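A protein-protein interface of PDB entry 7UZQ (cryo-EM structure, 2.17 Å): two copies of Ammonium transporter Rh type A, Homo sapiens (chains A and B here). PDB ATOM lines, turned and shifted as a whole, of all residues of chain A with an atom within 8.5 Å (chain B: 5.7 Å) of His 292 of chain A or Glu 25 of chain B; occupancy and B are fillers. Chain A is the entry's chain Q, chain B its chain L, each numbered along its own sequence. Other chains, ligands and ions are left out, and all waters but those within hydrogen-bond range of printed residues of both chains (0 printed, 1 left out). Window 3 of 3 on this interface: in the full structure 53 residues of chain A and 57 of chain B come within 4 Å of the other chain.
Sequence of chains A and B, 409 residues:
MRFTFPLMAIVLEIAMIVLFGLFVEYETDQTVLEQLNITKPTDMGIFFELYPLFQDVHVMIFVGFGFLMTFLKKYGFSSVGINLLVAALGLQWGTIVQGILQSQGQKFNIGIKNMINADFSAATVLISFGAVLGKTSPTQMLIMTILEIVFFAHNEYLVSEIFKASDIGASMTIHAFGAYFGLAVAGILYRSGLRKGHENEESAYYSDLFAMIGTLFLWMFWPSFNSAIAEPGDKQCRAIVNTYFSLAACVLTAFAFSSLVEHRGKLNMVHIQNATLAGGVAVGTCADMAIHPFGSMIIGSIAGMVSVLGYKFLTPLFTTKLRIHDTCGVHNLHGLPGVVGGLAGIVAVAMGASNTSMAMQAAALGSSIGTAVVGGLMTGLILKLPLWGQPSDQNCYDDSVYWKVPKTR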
ATOM      1  N   CYS A 237      -9.874 -19.639  -8.511  1.00  0.00           N
ATOM      2  CA  CYS A 237      -9.168 -18.948  -9.581  1.00  0.00           C
ATOM      3  C   CYS A 237     -10.072 -18.737 -10.788  1.00  0.00           C
ATOM      4  O   CYS A 237     -10.060 -17.663 -11.401  1.00  0.00           O
ATOM      5  CB  CYS A 237      -7.919 -19.737  -9.978  1.00  0.00           C
ATOM      6  SG  CYS A 237      -7.453 -19.544 -11.701  1.00  0.00           S
ATOM      7  N   ARG A 238     -10.859 -19.754 -11.144  1.00  0.00           N
ATOM      8  CA  ARG A 238     -11.787 -19.612 -12.257  1.00  0.00           C
ATOM      9  C   ARG A 238     -12.810 -18.522 -11.973  1.00  0.00           C
ATOM     10  O   ARG A 238     -13.152 -17.743 -12.863  1.00  0.00           O
ATOM     11  CB  ARG A 238     -12.487 -20.944 -12.537  1.00  0.00           C
ATOM     12  CG  ARG A 238     -11.731 -21.866 -13.484  1.00  0.00           C
ATOM     13  CD  ARG A 238     -12.679 -22.762 -14.265  1.00  0.00           C
ATOM     14  NE  ARG A 238     -13.576 -23.512 -13.394  1.00  0.00           N
ATOM     15  CZ  ARG A 238     -13.304 -24.689 -12.844  1.00  0.00           C
ATOM     16  NH1 ARG A 238     -12.146 -25.295 -13.036  1.00  0.00           N
ATOM     17  NH2 ARG A 238     -14.219 -25.271 -12.076  1.00  0.00           N
ATOM     18  N   VAL A 241     -11.068 -15.140 -12.535  1.00  0.00           N
ATOM     19  CA  VAL A 241     -10.764 -14.848 -13.936  1.00  0.00           C
ATOM     20  C   VAL A 241     -12.046 -14.574 -14.718  1.00  0.00           C
ATOM     21  O   VAL A 241     -12.125 -13.617 -15.506  1.00  0.00           O
ATOM     22  CB  VAL A 241      -9.947 -16.004 -14.546  1.00  0.00           C
ATOM     23  CG1 VAL A 241      -9.759 -15.811 -16.042  1.00  0.00           C
ATOM     24  CG2 VAL A 241      -8.597 -16.110 -13.858  1.00  0.00           C
ATOM     25  N   ASN A 242     -13.074 -15.400 -14.501  1.00  0.00           N
ATOM     26  CA  ASN A 242     -14.340 -15.232 -15.202  1.00  0.00           C
ATOM     27  C   ASN A 242     -14.986 -13.898 -14.862  1.00  0.00           C
ATOM     28  O   ASN A 242     -15.453 -13.184 -15.755  1.00  0.00           O
ATOM     29  CB  ASN A 242     -15.280 -16.387 -14.854  1.00  0.00           C
ATOM     30  CG  ASN A 242     -14.883 -17.684 -15.527  1.00  0.00           C
ATOM     31  OD1 ASN A 242     -14.266 -17.679 -16.588  1.00  0.00           O
ATOM     32  ND2 ASN A 242     -15.234 -18.802 -14.911  1.00  0.00           N
ATOM     33  N   THR A 243     -15.014 -13.536 -13.577  1.00  0.00           N
ATOM     34  CA  THR A 243     -15.600 -12.256 -13.196  1.00  0.00           C
ATOM     35  C   THR A 243     -14.831 -11.099 -13.817  1.00  0.00           C
ATOM     36  O   THR A 243     -15.427 -10.154 -14.349  1.00  0.00           O
ATOM     37  CB  THR A 243     -15.630 -12.137 -11.671  1.00  0.00           C
ATOM     38  OG1 THR A 243     -16.365 -13.235 -11.122  1.00  0.00           O
ATOM     39  CG2 THR A 243     -16.272 -10.827 -11.230  1.00  0.00           C
ATOM     40  N   PHE A 245     -12.934 -10.916 -16.610  1.00  0.00           N
ATOM     41  CA  PHE A 245     -13.131 -10.700 -18.038  1.00  0.00           C
ATOM     42  C   PHE A 245     -14.593 -10.429 -18.389  1.00  0.00           C
ATOM     43  O   PHE A 245     -14.867  -9.675 -19.333  1.00  0.00           O
ATOM     44  CB  PHE A 245     -12.559 -11.882 -18.820  1.00  0.00           C
ATOM     45  CG  PHE A 245     -11.053 -11.893 -18.858  1.00  0.00           C
ATOM     46  CD1 PHE A 245     -10.350 -10.871 -19.482  1.00  0.00           C
ATOM     47  CD2 PHE A 245     -10.340 -12.906 -18.248  1.00  0.00           C
ATOM     48  CE1 PHE A 245      -8.974 -10.872 -19.506  1.00  0.00           C
ATOM     49  CE2 PHE A 245      -8.958 -12.911 -18.270  1.00  0.00           C
ATOM     50  CZ  PHE A 245      -8.277 -11.898 -18.900  1.00  0.00           C
ATOM     51  N   SER A 246     -15.541 -10.981 -17.629  1.00  0.00           N
ATOM     52  CA  SER A 246     -16.947 -10.674 -17.858  1.00  0.00           C
ATOM     53  C   SER A 246     -17.227  -9.192 -17.638  1.00  0.00           C
ATOM     54  O   SER A 246     -17.899  -8.548 -18.452  1.00  0.00           O
ATOM     55  CB  SER A 246     -17.814 -11.530 -16.937  1.00  0.00           C
ATOM     56  OG  SER A 246     -19.179 -11.197 -17.058  1.00  0.00           O
ATOM     57  N   VAL A 283     -22.415 -13.237 -14.524  1.00  0.00           N
ATOM     58  CA  VAL A 283     -21.497 -14.373 -14.488  1.00  0.00           C
ATOM     59  C   VAL A 283     -21.475 -15.062 -13.133  1.00  0.00           C
ATOM     60  O   VAL A 283     -20.748 -16.047 -12.968  1.00  0.00           O
ATOM     61  CB  VAL A 283     -20.084 -13.896 -14.885  1.00  0.00           C
ATOM     62  CG1 VAL A 283     -19.350 -13.293 -13.690  1.00  0.00           C
ATOM     63  CG2 VAL A 283     -19.287 -15.027 -15.518  1.00  0.00           C
ATOM     64  N   CYS A 286     -22.296 -19.065 -12.868  1.00  0.00           N
ATOM     65  CA  CYS A 286     -21.290 -19.831 -13.653  1.00  0.00           C
ATOM     66  C   CYS A 286     -19.854 -19.465 -13.255  1.00  0.00           C
ATOM     67  O   CYS A 286     -18.945 -20.098 -13.810  1.00  0.00           O
ATOM     68  CB  CYS A 286     -21.453 -19.540 -15.141  1.00  0.00           C
ATOM     69  SG  CYS A 286     -23.035 -20.069 -15.840  1.00  0.00           S
ATOM     70  N   ALA A 287     -19.628 -18.487 -12.377  1.00  0.00           N
ATOM     71  CA  ALA A 287     -18.281 -17.942 -12.057  1.00  0.00           C
ATOM     72  C   ALA A 287     -17.238 -19.033 -11.758  1.00  0.00           C
ATOM     73  O   ALA A 287     -16.143 -18.903 -12.197  1.00  0.00           O
ATOM     74  CB  ALA A 287     -18.387 -16.978 -10.898  1.00  0.00           C
ATOM     75  N   ASP A 288     -17.542 -20.026 -10.945  1.00  0.00           N
ATOM     76  CA  ASP A 288     -16.608 -21.112 -10.670  1.00  0.00           C
ATOM     77  C   ASP A 288     -16.727 -22.273 -11.651  1.00  0.00           C
ATOM     78  O   ASP A 288     -15.971 -23.239 -11.533  1.00  0.00           O
ATOM     79  CB  ASP A 288     -16.790 -21.626  -9.238  1.00  0.00           C
ATOM     80  CG  ASP A 288     -18.181 -22.154  -8.968  1.00  0.00           C
ATOM     81  OD1 ASP A 288     -19.055 -22.059  -9.852  1.00  0.00           O
ATOM     82  OD2 ASP A 288     -18.401 -22.665  -7.854  1.00  0.00           O
ATOM     83  N   MET A 289     -17.658 -22.220 -12.591  1.00  0.00           N
ATOM     84  CA  MET A 289     -17.796 -23.268 -13.637  1.00  0.00           C
ATOM     85  C   MET A 289     -16.737 -23.051 -14.715  1.00  0.00           C
ATOM     86  O   MET A 289     -16.285 -21.906 -14.865  1.00  0.00           O
ATOM     87  CB  MET A 289     -19.177 -23.217 -14.284  1.00  0.00           C
ATOM     88  CG  MET A 289     -20.298 -23.347 -13.289  1.00  0.00           C
ATOM     89  SD  MET A 289     -21.898 -23.489 -14.098  1.00  0.00           S
ATOM     90  CE  MET A 289     -22.950 -23.716 -12.666  1.00  0.00           C
ATOM     91  N   ALA A 290     -16.356 -24.095 -15.447  1.00  0.00           N
ATOM     92  CA  ALA A 290     -15.389 -23.983 -16.566  1.00  0.00           C
ATOM     93  C   ALA A 290     -16.112 -23.586 -17.859  1.00  0.00           C
ATOM     94  O   ALA A 290     -16.182 -24.420 -18.771  1.00  0.00           O
ATOM     95  CB  ALA A 290     -14.631 -25.264 -16.713  1.00  0.00           C
ATOM     96  N   ILE A 291     -16.595 -22.353 -17.945  1.00  0.00           N
ATOM     97  CA  ILE A 291     -17.298 -21.827 -19.147  1.00  0.00           C
ATOM     98  C   ILE A 291     -16.261 -21.265 -20.115  1.00  0.00           C
ATOM     99  O   ILE A 291     -16.664 -20.889 -21.217  1.00  0.00           O
ATOM    100  CB  ILE A 291     -18.345 -20.782 -18.727  1.00  0.00           C
ATOM    101  CG1 ILE A 291     -17.714 -19.545 -18.080  1.00  0.00           C
ATOM    102  CG2 ILE A 291     -19.389 -21.414 -17.819  1.00  0.00           C
ATOM    103  CD1 ILE A 291     -18.590 -18.317 -18.143  1.00  0.00           C
ATOM    104  N   HIS A 292     -15.015 -21.118 -19.675  1.00  0.00           N
ATOM    105  CA  HIS A 292     -13.892 -20.562 -20.474  1.00  0.00           C
ATOM    106  C   HIS A 292     -13.908 -19.050 -20.266  1.00  0.00           C
ATOM    107  O   HIS A 292     -14.983 -18.501 -20.031  1.00  0.00           O
ATOM    108  CB  HIS A 292     -13.983 -20.955 -21.955  1.00  0.00           C
ATOM    109  CG  HIS A 292     -12.693 -20.925 -22.691  1.00  0.00           C
ATOM    110  ND1 HIS A 292     -12.191 -19.769 -23.249  1.00  0.00           N
ATOM    111  CD2 HIS A 292     -11.824 -21.908 -22.996  1.00  0.00           C
ATOM    112  CE1 HIS A 292     -11.054 -20.035 -23.849  1.00  0.00           C
ATOM    113  NE2 HIS A 292     -10.810 -21.343 -23.709  1.00  0.00           N
ATOM    114  N   PRO A 293     -12.787 -18.337 -20.445  1.00  0.00           N
ATOM    115  CA  PRO A 293     -12.793 -16.874 -20.402  1.00  0.00           C
ATOM    116  C   PRO A 293     -13.694 -16.297 -21.512  1.00  0.00           C
ATOM    117  O   PRO A 293     -14.326 -15.308 -21.268  1.00  0.00           O
ATOM    118  CB  PRO A 293     -11.307 -16.546 -20.588  1.00  0.00           C
ATOM    119  CG  PRO A 293     -10.621 -17.696 -19.915  1.00  0.00           C
ATOM    120  CD  PRO A 293     -11.424 -18.880 -20.397  1.00  0.00           C
ATOM    121  N   PHE A 294     -13.707 -16.891 -22.705  1.00  0.00           N
ATOM    122  CA  PHE A 294     -14.546 -16.428 -23.841  1.00  0.00           C
ATOM    123  C   PHE A 294     -16.031 -16.544 -23.451  1.00  0.00           C
ATOM    124  O   PHE A 294     -16.772 -15.600 -23.779  1.00  0.00           O
ATOM    125  CB  PHE A 294     -14.161 -17.160 -25.134  1.00  0.00           C
ATOM    126  CG  PHE A 294     -15.032 -18.312 -25.543  1.00  0.00           C
ATOM    127  CD1 PHE A 294     -16.305 -18.093 -26.037  1.00  0.00           C
ATOM    128  CD2 PHE A 294     -14.557 -19.610 -25.488  1.00  0.00           C
ATOM    129  CE1 PHE A 294     -17.105 -19.154 -26.424  1.00  0.00           C
ATOM    130  CE2 PHE A 294     -15.353 -20.668 -25.889  1.00  0.00           C
ATOM    131  CZ  PHE A 294     -16.626 -20.440 -26.354  1.00  0.00           C
ATOM    132  N   GLY A 295     -16.438 -17.617 -22.766  1.00  0.00           N
ATOM    133  CA  GLY A 295     -17.825 -17.791 -22.278  1.00  0.00           C
ATOM    134  C   GLY A 295     -18.209 -16.716 -21.271  1.00  0.00           C
ATOM    135  O   GLY A 295     -19.341 -16.222 -21.349  1.00  0.00           O
ATOM    136  N   SER A 296     -17.310 -16.345 -20.369  1.00  0.00           N
ATOM    137  CA  SER A 296     -17.558 -15.267 -19.381  1.00  0.00           C
ATOM    138  C   SER A 296     -17.751 -13.935 -20.117  1.00  0.00           C
ATOM    139  O   SER A 296     -18.640 -13.183 -19.713  1.00  0.00           O
ATOM    140  CB  SER A 296     -16.464 -15.241 -18.313  1.00  0.00           C
ATOM    141  OG  SER A 296     -15.290 -14.601 -18.788  1.00  0.00           O
ATOM    142  N   MET A 297     -16.958 -13.658 -21.149  1.00  0.00           N
ATOM    143  CA  MET A 297     -17.036 -12.411 -21.957  1.00  0.00           C
ATOM    144  C   MET A 297     -18.365 -12.304 -22.714  1.00  0.00           C
ATOM    145  O   MET A 297     -18.897 -11.207 -22.794  1.00  0.00           O
ATOM    146  CB  MET A 297     -15.867 -12.342 -22.935  1.00  0.00           C
ATOM    147  CG  MET A 297     -14.612 -11.828 -22.277  1.00  0.00           C
ATOM    148  SD  MET A 297     -13.114 -12.497 -23.011  1.00  0.00           S
ATOM    149  CE  MET A 297     -13.028 -11.531 -24.515  1.00  0.00           C
ATOM    150  N   ILE A 298     -18.849 -13.407 -23.280  1.00  0.00           N
ATOM    151  CA  ILE A 298     -20.142 -13.428 -24.007  1.00  0.00           C
ATOM    152  C   ILE A 298     -21.277 -13.094 -23.041  1.00  0.00           C
ATOM    153  O   ILE A 298     -22.084 -12.233 -23.383  1.00  0.00           O
ATOM    154  CB  ILE A 298     -20.350 -14.822 -24.617  1.00  0.00           C
ATOM    155  CG1 ILE A 298     -19.407 -15.099 -25.786  1.00  0.00           C
ATOM    156  CG2 ILE A 298     -21.809 -15.015 -25.007  1.00  0.00           C
ATOM    157  CD1 ILE A 298     -19.168 -16.570 -26.004  1.00  0.00           C
ATOM    158  N   ILE A 299     -21.267 -13.682 -21.845  1.00  0.00           N
ATOM    159  CA  ILE A 299     -22.280 -13.389 -20.803  1.00  0.00           C
ATOM    160  C   ILE A 299     -22.156 -11.927 -20.384  1.00  0.00           C
ATOM    161  O   ILE A 299     -23.185 -11.265 -20.309  1.00  0.00           O
ATOM    162  CB  ILE A 299     -22.088 -14.332 -19.605  1.00  0.00           C
ATOM    163  CG1 ILE A 299     -22.538 -15.760 -19.922  1.00  0.00           C
ATOM    164  CG2 ILE A 299     -22.775 -13.784 -18.361  1.00  0.00           C
ATOM    165  CD1 ILE A 299     -21.863 -16.805 -19.076  1.00  0.00           C
ATOM    166  N   ALA A 353     -20.462 -28.157 -18.398  1.00  0.00           N
ATOM    167  CA  ALA A 353     -19.478 -27.256 -17.774  1.00  0.00           C
ATOM    168  C   ALA A 353     -19.513 -27.557 -16.292  1.00  0.00           C
ATOM    169  O   ALA A 353     -18.441 -27.521 -15.662  1.00  0.00           O
ATOM    170  CB  ALA A 353     -19.781 -25.804 -18.057  1.00  0.00           C
ATOM    171  N   PHE B  20     -10.038 -14.593 -27.569  1.00  0.00           N
ATOM    172  CA  PHE B  20      -9.968 -15.355 -26.330  1.00  0.00           C
ATOM    173  C   PHE B  20     -10.354 -16.806 -26.569  1.00  0.00           C
ATOM    174  O   PHE B  20      -9.711 -17.720 -26.048  1.00  0.00           O
ATOM    175  CB  PHE B  20     -10.859 -14.722 -25.264  1.00  0.00           C
ATOM    176  CG  PHE B  20     -10.141 -13.755 -24.371  1.00  0.00           C
ATOM    177  CD1 PHE B  20      -9.711 -12.533 -24.855  1.00  0.00           C
ATOM    178  CD2 PHE B  20      -9.904 -14.060 -23.044  1.00  0.00           C
ATOM    179  CE1 PHE B  20      -9.057 -11.638 -24.032  1.00  0.00           C
ATOM    180  CE2 PHE B  20      -9.246 -13.167 -22.217  1.00  0.00           C
ATOM    181  CZ  PHE B  20      -8.824 -11.956 -22.715  1.00  0.00           C
ATOM    182  N   GLY B  21     -11.388 -17.035 -27.379  1.00  0.00           N
ATOM    183  CA  GLY B  21     -11.751 -18.398 -27.717  1.00  0.00           C
ATOM    184  C   GLY B  21     -10.642 -19.136 -28.437  1.00  0.00           C
ATOM    185  O   GLY B  21     -10.465 -20.340 -28.245  1.00  0.00           O
ATOM    186  N   PHE B  23      -7.221 -18.472 -28.296  1.00  0.00           N
ATOM    187  CA  PHE B  23      -5.865 -18.437 -27.766  1.00  0.00           C
ATOM    188  C   PHE B  23      -5.724 -18.654 -26.265  1.00  0.00           C
ATOM    189  O   PHE B  23      -4.593 -18.826 -25.802  1.00  0.00           O
ATOM    190  CB  PHE B  23      -5.207 -17.092 -28.111  1.00  0.00           C
ATOM    191  CG  PHE B  23      -4.853 -16.943 -29.557  1.00  0.00           C
ATOM    192  CD1 PHE B  23      -3.789 -17.645 -30.098  1.00  0.00           C
ATOM    193  CD2 PHE B  23      -5.572 -16.094 -30.374  1.00  0.00           C
ATOM    194  CE1 PHE B  23      -3.458 -17.505 -31.424  1.00  0.00           C
ATOM    195  CE2 PHE B  23      -5.243 -15.950 -31.701  1.00  0.00           C
ATOM    196  CZ  PHE B  23      -4.186 -16.655 -32.228  1.00  0.00           C
ATOM    197  N   VAL B  24      -6.806 -18.662 -25.492  1.00  0.00           N
ATOM    198  CA  VAL B  24      -6.725 -18.549 -24.040  1.00  0.00           C
ATOM    199  C   VAL B  24      -7.277 -19.808 -23.384  1.00  0.00           C
ATOM    200  O   VAL B  24      -8.221 -20.424 -23.887  1.00  0.00           O
ATOM    201  CB  VAL B  24      -7.473 -17.292 -23.550  1.00  0.00           C
ATOM    202  CG1 VAL B  24      -7.613 -17.292 -22.045  1.00  0.00           C
ATOM    203  CG2 VAL B  24      -6.756 -16.044 -24.015  1.00  0.00           C
ATOM    204  N   GLU B  25      -6.708 -20.200 -22.239  1.00  0.00           N
ATOM    205  CA  GLU B  25      -7.208 -21.326 -21.408  1.00  0.00           C
ATOM    206  C   GLU B  25      -7.008 -20.917 -19.949  1.00  0.00           C
ATOM    207  O   GLU B  25      -6.250 -19.963 -19.720  1.00  0.00           O
ATOM    208  CB  GLU B  25      -6.471 -22.630 -21.699  1.00  0.00           C
ATOM    209  CG  GLU B  25      -6.635 -23.109 -23.129  1.00  0.00           C
ATOM    210  CD  GLU B  25      -8.050 -23.530 -23.486  1.00  0.00           C
ATOM    211  OE1 GLU B  25      -8.888 -23.613 -22.571  1.00  0.00           O
ATOM    212  OE2 GLU B  25      -8.309 -23.778 -24.679  1.00  0.00           O
ATOM    213  N   TYR B  26      -7.664 -21.576 -18.999  1.00  0.00           N
ATOM    214  CA  TYR B  26      -7.453 -21.298 -17.559  1.00  0.00           C
ATOM    215  C   TYR B  26      -6.064 -21.832 -17.178  1.00  0.00           C
ATOM    216  O   TYR B  26      -5.378 -21.153 -16.398  1.00  0.00           O
ATOM    217  CB  TYR B  26      -8.547 -21.920 -16.686  1.00  0.00           C
ATOM    218  CG  TYR B  26      -9.957 -21.430 -16.880  1.00  0.00           C
ATOM    219  CD1 TYR B  26     -10.339 -20.152 -16.508  1.00  0.00           C
ATOM    220  CD2 TYR B  26     -10.931 -22.283 -17.367  1.00  0.00           C
ATOM    221  CE1 TYR B  26     -11.647 -19.722 -16.657  1.00  0.00           C
ATOM    222  CE2 TYR B  26     -12.239 -21.870 -17.526  1.00  0.00           C
ATOM    223  CZ  TYR B  26     -12.599 -20.587 -17.165  1.00  0.00           C
ATOM    224  OH  TYR B  26     -13.892 -20.195 -17.330  1.00  0.00           O
ATOM    225  N   LYS B 107      -1.465 -21.288 -27.892  1.00  0.00           N
ATOM    226  CA  LYS B 107      -2.379 -21.079 -26.786  1.00  0.00           C
ATOM    227  C   LYS B 107      -1.581 -20.853 -25.507  1.00  0.00           C
ATOM    228  O   LYS B 107      -0.429 -21.274 -25.380  1.00  0.00           O
ATOM    229  CB  LYS B 107      -3.311 -22.277 -26.617  1.00  0.00           C
ATOM    230  CG  LYS B 107      -4.464 -22.331 -27.604  1.00  0.00           C
ATOM    231  CD  LYS B 107      -5.702 -22.942 -26.970  1.00  0.00           C
ATOM    232  CE  LYS B 107      -6.753 -23.317 -28.006  1.00  0.00           C
ATOM    233  NZ  LYS B 107      -8.033 -22.597 -27.773  1.00  0.00           N
ATOM    234  N   PHE B 108      -2.202 -20.165 -24.556  1.00  0.00           N
ATOM    235  CA  PHE B 108      -1.549 -19.856 -23.296  1.00  0.00           C
ATOM    236  C   PHE B 108      -2.598 -19.803 -22.198  1.00  0.00           C
ATOM    237  O   PHE B 108      -3.789 -19.628 -22.457  1.00  0.00           O
ATOM    238  CB  PHE B 108      -0.769 -18.534 -23.377  1.00  0.00           C
ATOM    239  CG  PHE B 108      -1.638 -17.324 -23.546  1.00  0.00           C
ATOM    240  CD1 PHE B 108      -2.090 -16.617 -22.445  1.00  0.00           C
ATOM    241  CD2 PHE B 108      -1.995 -16.882 -24.807  1.00  0.00           C
ATOM    242  CE1 PHE B 108      -2.890 -15.508 -22.597  1.00  0.00           C
ATOM    243  CE2 PHE B 108      -2.793 -15.769 -24.960  1.00  0.00           C
ATOM    244  CZ  PHE B 108      -3.242 -15.083 -23.854  1.00  0.00           C
ATOM    245  N   ASN B 109      -2.134 -19.959 -20.965  1.00  0.00           N
ATOM    246  CA  ASN B 109      -2.986 -19.964 -19.787  1.00  0.00           C
ATOM    247  C   ASN B 109      -3.015 -18.584 -19.147  1.00  0.00           C
ATOM    248  O   ASN B 109      -2.100 -17.775 -19.318  1.00  0.00           O
ATOM    249  CB  ASN B 109      -2.499 -21.003 -18.776  1.00  0.00           C
ATOM    250  CG  ASN B 109      -2.263 -22.357 -19.405  1.00  0.00           C
ATOM    251  OD1 ASN B 109      -3.100 -22.863 -20.147  1.00  0.00           O
ATOM    252  ND2 ASN B 109      -1.115 -22.952 -19.110  1.00  0.00           N
ATOM    253  N   ILE B 110      -4.085 -18.322 -18.407  1.00  0.00           N
ATOM    254  CA  ILE B 110      -4.306 -17.033 -17.762  1.00  0.00           C
ATOM    255  C   ILE B 110      -4.072 -17.217 -16.274  1.00  0.00           C
ATOM    256  O   ILE B 110      -4.860 -17.876 -15.585  1.00  0.00           O
ATOM    257  CB  ILE B 110      -5.712 -16.484 -18.034  1.00  0.00           C
ATOM    258  CG1 ILE B 110      -5.843 -16.066 -19.497  1.00  0.00           C
ATOM    259  CG2 ILE B 110      -6.029 -15.315 -17.092  1.00  0.00           C
ATOM    260  CD1 ILE B 110      -5.004 -14.873 -19.912  1.00  0.00           C
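Along chain A the printed residues that touch a printed residue of chain B span positions 238 to 297. Printed residues of chain B that touch a printed residue of chain A: Phe 20, Gly 21, Val 24, Glu 25, Tyr 26 and Ile 110. Hydrophobic or aromatic side chains of chain B within 4 Å of the printed part of chain A: Phe 20, Val 24, Tyr 26 and Ile 110. Along chain B the printed residues that touch a printed residue of chain A span positions 20 to 110. Among the printed residues, no Asp or Glu carboxylate lies within 4 Å of a Lys or Arg side-chain nitrogen of the other chain.
A ring nitrogen (ND1) of His 292 of chain A lies close to the backbone NH of Phe 294 of chain A, 3.3 Å away. ND2 of Asn 242 of chain A lies within hydrogen-bond range of O of Arg 238 of chain A, at 3.1 Å. The backbone carbonyl oxygen (O) of Phe 108 of chain B lies within hydrogen-bond range of the backbone NH (N) of Glu 25 of chain B, 3.0 Å away. The guanidinium group (NH2) of Arg 238 of chain A is in hydrogen-bond range of the backbone carbonyl oxygen (O) of Asp 288 of chain A (2.7 Å). The backbone carbonyl oxygen (O) of Ala 287 of chain A is in hydrogen-bond range of the side-chain amide nitrogen (ND2) of Asn 242 of chain A. O of Asn 242 of chain A is in hydrogen-bond range of OG of Ser 296 of chain A (3.4 Å).
Of the printed residues of chain B, Arg 238 of chain A touches Tyr 26. His 292 of chain A touches just these residues of chain B: Phe 20 (3.5 Å), Val 24 (2.8 Å), Glu 25 (3.2 Å) and Tyr 26 (2.8 Å). Of the printed residues of chain B, Pro 293 of chain A touches Phe 20, Val 24 and Tyr 26. Printed residues of chain B within 4 Å of Phe 294 of chain A: Gly 21 (3.6 Å). Printed residues of chain B within 4 Å of Met 297 of chain A: Phe 20. Of chain A, only His 292 (3.2 Å) comes within 4 Å of Glu 25 of chain B. Of the printed residues of chain A, Ile 110 of chain B touches Val 241 and Phe 245. The nearest residue of chain A that does not touch Glu 25 of chain B is Pro 293 of chain A (4.8 Å).
CD of Arg 238 of chain A touches CE2 of Tyr 26 of chain B (3.4 Å). Ile 110 of chain B touches Val 241 of chain A (CG2 to CG1, 3.9 Å). CE2 of Phe 245 of chain A touches CG2 of Ile 110 of chain B (3.97 Å). Met 289 of chain A touches Tyr 26 of chain B. Ala 290 of chain A touches Tyr 26 of chain B (CA to CE2, 3.9 Å). Ile 291 of chain A touches Tyr 26 of chain B (N to OH, 3.5 Å). CE1 of His 292 of chain A touches O of Phe 20 of chain B (3.5 Å). CB of Pro 293 of chain A touches CD2 of Phe 20 of chain B, at 3.8 Å. Phe 294 of chain A touches Gly 21 of chain B (CB to N, 3.6 Å). Met 297 of chain A touches Phe 20 of chain B.
No position is printed for both chains. Of the 17 pairs that touch across the chains among the printed residues, none has its exchanged pair printed and touching as well.
The side-chain hydroxyl of Tyr 26 of chain B is in hydrogen-bond range of the backbone NH of His 292 of chain A (2.8 Å). OE1 of Glu 25 of chain B lies within hydrogen-bond range of NE2 of His 292 of chain A (3.2 Å). OH of Tyr 26 of chain B lies within hydrogen-bond range of OD1 of Asn 242 of chain A. A ring nitrogen (NE2) of His 292 of chain A lies within hydrogen-bond range of the backbone carbonyl oxygen of Val 24 of chain B, at 2.8 Å.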
